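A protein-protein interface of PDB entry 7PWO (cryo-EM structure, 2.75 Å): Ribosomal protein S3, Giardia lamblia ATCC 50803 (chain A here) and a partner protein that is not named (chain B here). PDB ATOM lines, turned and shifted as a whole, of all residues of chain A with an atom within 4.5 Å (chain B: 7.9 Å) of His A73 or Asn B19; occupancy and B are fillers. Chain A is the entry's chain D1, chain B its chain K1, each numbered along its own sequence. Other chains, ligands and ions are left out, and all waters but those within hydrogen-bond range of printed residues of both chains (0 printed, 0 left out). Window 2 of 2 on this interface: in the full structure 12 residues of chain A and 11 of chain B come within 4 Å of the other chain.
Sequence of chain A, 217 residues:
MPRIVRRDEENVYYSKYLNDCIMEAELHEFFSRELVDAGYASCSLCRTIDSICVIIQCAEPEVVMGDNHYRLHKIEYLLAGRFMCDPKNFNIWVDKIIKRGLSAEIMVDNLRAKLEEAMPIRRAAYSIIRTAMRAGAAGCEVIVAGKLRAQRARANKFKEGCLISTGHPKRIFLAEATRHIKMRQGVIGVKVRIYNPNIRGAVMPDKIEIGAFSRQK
Asn B19 touches just these residues of chain A: His A73, Lys A74 and Tyr A77. Lys A74 touches just these residues of chain B: Asn B19 (3.6 Å) and Ser B21 (3.2 Å). Of the printed residues of chain A, Leu B79 touches Tyr A70 (3.5 Å). Of the printed residues of chain A, Glu B18 touches Tyr A70. Of the printed residues of chain A, Ser B21 touches Lys A74. Of the printed residues of chain B, Tyr A77 touches Asn B19 (2.9 Å). Of the printed residues of chain B, Tyr A70 touches Glu B18 (3.8 Å) and Leu B79 (3.5 Å). Ile A75 touches none of the printed residues of chain B. His B15 touches none of the printed residues of chain A. The nearest printed residue of chain A that does not touch Glu B18 is Tyr A77 (4.6 Å).
Among the printed residues, merely in contact across the chains: Tyr A77 with Asn B19, His A73 with Asn B19, Tyr A70 with Leu B79, Lys A74 with Asn B19 and Tyr A70 with Glu B18.
Printed residues of chain B that touch a printed residue of chain A: Glu B18, Asn B19, Ser B21 and Leu B79. Hydrophobic or aromatic side chains of chain B within 4 Å of the printed part of chain A: Leu B79. Hydrophobic or aromatic side chains of chain A within 4 Å of the printed part of chain B: Tyr A70, His A73 and Tyr A77.
OG of Ser B21 is in hydrogen-bond range of O of Lys A74, 3.2 Å away.
OE2 of Glu B18 sits close to OD1 of Asn B19 (3.2 Å). The backbone carbonyl oxygen (O) of His A69 sits at hydrogen-bond distance from a ring nitrogen (ND1) of His A73 (2.8 Å).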
ATOM      1  N   HIS A  69      14.923  14.828 -15.076  1.00  0.00           N
ATOM      2  CA  HIS A  69      14.029  15.786 -15.717  1.00  0.00           C
ATOM      3  C   HIS A  69      12.591  15.276 -15.808  1.00  0.00           C
ATOM      4  O   HIS A  69      11.750  15.941 -16.435  1.00  0.00           O
ATOM      5  CB  HIS A  69      14.517  16.169 -17.119  1.00  0.00           C
ATOM      6  CG  HIS A  69      15.742  17.033 -17.124  1.00  0.00           C
ATOM      7  ND1 HIS A  69      16.382  17.403 -18.288  1.00  0.00           N
ATOM      8  CD2 HIS A  69      16.443  17.598 -16.112  1.00  0.00           C
ATOM      9  CE1 HIS A  69      17.425  18.158 -17.992  1.00  0.00           C
ATOM     10  NE2 HIS A  69      17.485  18.291 -16.679  1.00  0.00           N
ATOM     11  N   TYR A  70      12.289  14.120 -15.210  1.00  0.00           N
ATOM     12  CA  TYR A  70      10.986  13.469 -15.336  1.00  0.00           C
ATOM     13  C   TYR A  70       9.844  14.422 -15.008  1.00  0.00           C
ATOM     14  O   TYR A  70       8.887  14.547 -15.779  1.00  0.00           O
ATOM     15  CB  TYR A  70      10.958  12.245 -14.418  1.00  0.00           C
ATOM     16  CG  TYR A  70       9.652  11.487 -14.325  1.00  0.00           C
ATOM     17  CD1 TYR A  70       9.019  10.992 -15.455  1.00  0.00           C
ATOM     18  CD2 TYR A  70       9.058  11.251 -13.087  1.00  0.00           C
ATOM     19  CE1 TYR A  70       7.833  10.285 -15.357  1.00  0.00           C
ATOM     20  CE2 TYR A  70       7.859  10.552 -12.981  1.00  0.00           C
ATOM     21  CZ  TYR A  70       7.252  10.073 -14.116  1.00  0.00           C
ATOM     22  OH  TYR A  70       6.063   9.374 -14.012  1.00  0.00           O
ATOM     23  N   ARG A  71       9.939  15.115 -13.872  1.00  0.00           N
ATOM     24  CA  ARG A  71       8.881  16.039 -13.469  1.00  0.00           C
ATOM     25  C   ARG A  71       8.752  17.216 -14.434  1.00  0.00           C
ATOM     26  O   ARG A  71       7.635  17.653 -14.733  1.00  0.00           O
ATOM     27  CB  ARG A  71       9.124  16.525 -12.038  1.00  0.00           C
ATOM     28  CG  ARG A  71      10.250  17.529 -11.876  1.00  0.00           C
ATOM     29  CD  ARG A  71      10.496  17.860 -10.419  1.00  0.00           C
ATOM     30  NE  ARG A  71       9.536  18.823  -9.881  1.00  0.00           N
ATOM     31  CZ  ARG A  71       8.599  18.530  -8.980  1.00  0.00           C
ATOM     32  NH1 ARG A  71       8.482  17.295  -8.516  1.00  0.00           N
ATOM     33  NH2 ARG A  71       7.777  19.478  -8.542  1.00  0.00           N
ATOM     34  N   LEU A  72       9.872  17.747 -14.931  1.00  0.00           N
ATOM     35  CA  LEU A  72       9.805  18.869 -15.865  1.00  0.00           C
ATOM     36  C   LEU A  72       9.129  18.466 -17.169  1.00  0.00           C
ATOM     37  O   LEU A  72       8.301  19.213 -17.713  1.00  0.00           O
ATOM     38  CB  LEU A  72      11.204  19.406 -16.141  1.00  0.00           C
ATOM     39  CG  LEU A  72      11.268  20.442 -17.265  1.00  0.00           C
ATOM     40  CD1 LEU A  72      10.638  21.760 -16.829  1.00  0.00           C
ATOM     41  CD2 LEU A  72      12.694  20.620 -17.785  1.00  0.00           C
ATOM     42  N   HIS A  73       9.471  17.289 -17.692  1.00  0.00           N
ATOM     43  CA  HIS A  73       8.782  16.799 -18.880  1.00  0.00           C
ATOM     44  C   HIS A  73       7.311  16.532 -18.600  1.00  0.00           C
ATOM     45  O   HIS A  73       6.454  16.794 -19.453  1.00  0.00           O
ATOM     46  CB  HIS A  73       9.458  15.543 -19.422  1.00  0.00           C
ATOM     47  CG  HIS A  73      10.836  15.776 -19.958  1.00  0.00           C
ATOM     48  ND1 HIS A  73      11.971  15.705 -19.181  1.00  0.00           N
ATOM     49  CD2 HIS A  73      11.257  16.081 -21.209  1.00  0.00           C
ATOM     50  CE1 HIS A  73      13.030  15.951 -19.933  1.00  0.00           C
ATOM     51  NE2 HIS A  73      12.625  16.183 -21.166  1.00  0.00           N
ATOM     52  N   LYS A  74       7.001  15.996 -17.419  1.00  0.00           N
ATOM     53  CA  LYS A  74       5.608  15.746 -17.086  1.00  0.00           C
ATOM     54  C   LYS A  74       4.822  17.052 -17.050  1.00  0.00           C
ATOM     55  O   LYS A  74       3.668  17.105 -17.489  1.00  0.00           O
ATOM     56  CB  LYS A  74       5.527  15.004 -15.754  1.00  0.00           C
ATOM     57  N   ILE A  75       5.448  18.128 -16.572  1.00  0.00           N
ATOM     58  CA  ILE A  75       4.794  19.433 -16.584  1.00  0.00           C
ATOM     59  C   ILE A  75       4.579  19.917 -18.016  1.00  0.00           C
ATOM     60  O   ILE A  75       3.474  20.347 -18.375  1.00  0.00           O
ATOM     61  CB  ILE A  75       5.590  20.455 -15.752  1.00  0.00           C
ATOM     62  CG1 ILE A  75       5.718  19.985 -14.300  1.00  0.00           C
ATOM     63  CG2 ILE A  75       4.922  21.812 -15.795  1.00  0.00           C
ATOM     64  CD1 ILE A  75       4.381  19.822 -13.592  1.00  0.00           C
ATOM     65  N   GLU A  76       5.628  19.868 -18.851  1.00  0.00           N
ATOM     66  CA  GLU A  76       5.472  20.280 -20.249  1.00  0.00           C
ATOM     67  C   GLU A  76       4.326  19.546 -20.924  1.00  0.00           C
ATOM     68  O   GLU A  76       3.574  20.132 -21.713  1.00  0.00           O
ATOM     69  CB  GLU A  76       6.780  20.064 -21.022  1.00  0.00           C
ATOM     70  CG  GLU A  76       6.758  20.539 -22.491  1.00  0.00           C
ATOM     71  CD  GLU A  76       6.715  22.056 -22.678  1.00  0.00           C
ATOM     72  OE1 GLU A  76       6.284  22.769 -21.758  1.00  0.00           O
ATOM     73  OE2 GLU A  76       7.109  22.539 -23.757  1.00  0.00           O
ATOM     74  N   TYR A  77       4.178  18.259 -20.630  1.00  0.00           N
ATOM     75  CA  TYR A  77       3.080  17.524 -21.229  1.00  0.00           C
ATOM     76  C   TYR A  77       1.772  17.711 -20.479  1.00  0.00           C
ATOM     77  O   TYR A  77       0.740  17.207 -20.931  1.00  0.00           O
ATOM     78  CB  TYR A  77       3.447  16.053 -21.367  1.00  0.00           C
ATOM     79  CG  TYR A  77       4.526  15.848 -22.397  1.00  0.00           C
ATOM     80  CD1 TYR A  77       4.859  16.851 -23.305  1.00  0.00           C
ATOM     81  CD2 TYR A  77       5.197  14.654 -22.487  1.00  0.00           C
ATOM     82  CE1 TYR A  77       5.840  16.671 -24.263  1.00  0.00           C
ATOM     83  CE2 TYR A  77       6.194  14.460 -23.445  1.00  0.00           C
ATOM     84  CZ  TYR A  77       6.512  15.480 -24.326  1.00  0.00           C
ATOM     85  OH  TYR A  77       7.495  15.286 -25.273  1.00  0.00           O
ATOM     86  N   TYR B  13      -5.279   6.816 -20.649  1.00  0.00           N
ATOM     87  CA  TYR B  13      -4.633   8.126 -20.800  1.00  0.00           C
ATOM     88  C   TYR B  13      -3.466   8.342 -19.799  1.00  0.00           C
ATOM     89  O   TYR B  13      -2.977   9.457 -19.638  1.00  0.00           O
ATOM     90  CB  TYR B  13      -5.653   9.272 -20.740  1.00  0.00           C
ATOM     91  CG  TYR B  13      -5.135  10.552 -21.396  1.00  0.00           C
ATOM     92  CD1 TYR B  13      -4.433  11.509 -20.664  1.00  0.00           C
ATOM     93  CD2 TYR B  13      -5.424  10.842 -22.728  1.00  0.00           C
ATOM     94  CE1 TYR B  13      -3.963  12.664 -21.247  1.00  0.00           C
ATOM     95  CE2 TYR B  13      -4.951  12.003 -23.324  1.00  0.00           C
ATOM     96  CZ  TYR B  13      -4.234  12.918 -22.569  1.00  0.00           C
ATOM     97  OH  TYR B  13      -3.772  14.085 -23.132  1.00  0.00           O
ATOM     98  N   ALA B  14      -2.935   7.289 -19.182  1.00  0.00           N
ATOM     99  CA  ALA B  14      -1.702   7.389 -18.405  1.00  0.00           C
ATOM    100  C   ALA B  14      -0.602   6.583 -19.092  1.00  0.00           C
ATOM    101  O   ALA B  14      -0.594   5.349 -19.019  1.00  0.00           O
ATOM    102  CB  ALA B  14      -1.917   6.904 -16.971  1.00  0.00           C
ATOM    103  N   HIS B  15       0.324   7.277 -19.757  1.00  0.00           N
ATOM    104  CA  HIS B  15       1.565   6.655 -20.218  1.00  0.00           C
ATOM    105  C   HIS B  15       2.427   6.282 -19.017  1.00  0.00           C
ATOM    106  O   HIS B  15       2.863   7.161 -18.265  1.00  0.00           O
ATOM    107  CB  HIS B  15       2.337   7.593 -21.136  1.00  0.00           C
ATOM    108  CG  HIS B  15       1.752   7.741 -22.501  1.00  0.00           C
ATOM    109  ND1 HIS B  15       2.132   8.748 -23.364  1.00  0.00           N
ATOM    110  CD2 HIS B  15       0.831   7.004 -23.164  1.00  0.00           C
ATOM    111  CE1 HIS B  15       1.462   8.629 -24.496  1.00  0.00           C
ATOM    112  NE2 HIS B  15       0.668   7.578 -24.402  1.00  0.00           N
ATOM    113  N   LEU B  16       2.702   4.987 -18.854  1.00  0.00           N
ATOM    114  CA  LEU B  16       3.109   4.485 -17.543  1.00  0.00           C
ATOM    115  C   LEU B  16       4.533   4.892 -17.184  1.00  0.00           C
ATOM    116  O   LEU B  16       4.758   5.596 -16.195  1.00  0.00           O
ATOM    117  CB  LEU B  16       2.966   2.969 -17.505  1.00  0.00           C
ATOM    118  CG  LEU B  16       1.627   2.618 -16.885  1.00  0.00           C
ATOM    119  CD1 LEU B  16       1.366   1.133 -16.972  1.00  0.00           C
ATOM    120  CD2 LEU B  16       1.666   3.112 -15.469  1.00  0.00           C
ATOM    121  N   TYR B  17       5.510   4.453 -17.970  1.00  0.00           N
ATOM    122  CA  TYR B  17       6.889   4.850 -17.757  1.00  0.00           C
ATOM    123  C   TYR B  17       7.210   6.152 -18.471  1.00  0.00           C
ATOM    124  O   TYR B  17       8.262   6.750 -18.218  1.00  0.00           O
ATOM    125  CB  TYR B  17       7.818   3.737 -18.245  1.00  0.00           C
ATOM    126  CG  TYR B  17       9.258   3.826 -17.791  1.00  0.00           C
ATOM    127  CD1 TYR B  17       9.616   3.519 -16.488  1.00  0.00           C
ATOM    128  CD2 TYR B  17      10.262   4.193 -18.681  1.00  0.00           C
ATOM    129  CE1 TYR B  17      10.937   3.581 -16.077  1.00  0.00           C
ATOM    130  CE2 TYR B  17      11.581   4.262 -18.281  1.00  0.00           C
ATOM    131  CZ  TYR B  17      11.914   3.959 -16.977  1.00  0.00           C
ATOM    132  OH  TYR B  17      13.219   4.023 -16.573  1.00  0.00           O
ATOM    133  N   GLU B  18       6.313   6.602 -19.343  1.00  0.00           N
ATOM    134  CA  GLU B  18       6.460   7.834 -20.094  1.00  0.00           C
ATOM    135  C   GLU B  18       5.859   8.914 -19.202  1.00  0.00           C
ATOM    136  O   GLU B  18       5.615   8.664 -18.019  1.00  0.00           O
ATOM    137  CB  GLU B  18       5.766   7.707 -21.455  1.00  0.00           C
ATOM    138  CG  GLU B  18       5.898   8.883 -22.395  1.00  0.00           C
ATOM    139  CD  GLU B  18       7.345   9.051 -22.813  1.00  0.00           C
ATOM    140  OE1 GLU B  18       8.070   8.031 -22.786  1.00  0.00           O
ATOM    141  OE2 GLU B  18       7.751  10.176 -23.179  1.00  0.00           O
ATOM    142  N   ASN B  19       5.597  10.109 -19.730  1.00  0.00           N
ATOM    143  CA  ASN B  19       5.306  11.267 -18.896  1.00  0.00           C
ATOM    144  C   ASN B  19       4.089  12.074 -19.355  1.00  0.00           C
ATOM    145  O   ASN B  19       4.096  13.303 -19.226  1.00  0.00           O
ATOM    146  CB  ASN B  19       6.565  12.138 -18.829  1.00  0.00           C
ATOM    147  CG  ASN B  19       7.153  12.401 -20.202  1.00  0.00           C
ATOM    148  OD1 ASN B  19       6.445  12.346 -21.201  1.00  0.00           O
ATOM    149  ND2 ASN B  19       8.449  12.670 -20.260  1.00  0.00           N
ATOM    150  N   ALA B  20       3.059  11.435 -19.905  1.00  0.00           N
ATOM    151  CA  ALA B  20       1.775  12.100 -20.083  1.00  0.00           C
ATOM    152  C   ALA B  20       1.190  12.520 -18.734  1.00  0.00           C
ATOM    153  O   ALA B  20       1.541  11.976 -17.684  1.00  0.00           O
ATOM    154  CB  ALA B  20       0.796  11.181 -20.809  1.00  0.00           C
ATOM    155  N   SER B  21       0.296  13.513 -18.767  1.00  0.00           N
ATOM    156  CA  SER B  21      -0.389  14.004 -17.578  1.00  0.00           C
ATOM    157  C   SER B  21      -1.826  14.374 -17.929  1.00  0.00           C
ATOM    158  O   SER B  21      -2.129  14.733 -19.068  1.00  0.00           O
ATOM    159  CB  SER B  21       0.337  15.206 -16.958  1.00  0.00           C
ATOM    160  OG  SER B  21       1.627  14.858 -16.482  1.00  0.00           O
ATOM    161  N   LEU B  22      -2.713  14.286 -16.929  1.00  0.00           N
ATOM    162  CA  LEU B  22      -4.150  14.396 -17.143  1.00  0.00           C
ATOM    163  C   LEU B  22      -4.718  15.681 -16.538  1.00  0.00           C
ATOM    164  O   LEU B  22      -4.268  16.154 -15.485  1.00  0.00           O
ATOM    165  CB  LEU B  22      -4.870  13.172 -16.557  1.00  0.00           C
ATOM    166  CG  LEU B  22      -6.362  12.926 -16.790  1.00  0.00           C
ATOM    167  CD1 LEU B  22      -6.623  11.440 -16.700  1.00  0.00           C
ATOM    168  CD2 LEU B  22      -7.277  13.678 -15.828  1.00  0.00           C
ATOM    169  N   LEU B  79       1.102  11.971 -11.713  1.00  0.00           N
ATOM    170  CA  LEU B  79       1.227  10.567 -11.347  1.00  0.00           C
ATOM    171  C   LEU B  79       2.451  10.348 -10.473  1.00  0.00           C
ATOM    172  O   LEU B  79       3.518  10.926 -10.705  1.00  0.00           O
ATOM    173  CB  LEU B  79       1.315   9.671 -12.584  1.00  0.00           C
ATOM    174  CG  LEU B  79       2.598   9.645 -13.430  1.00  0.00           C
ATOM    175  CD1 LEU B  79       2.576   8.437 -14.342  1.00  0.00           C
ATOM    176  CD2 LEU B  79       2.825  10.927 -14.233  1.00  0.00           C
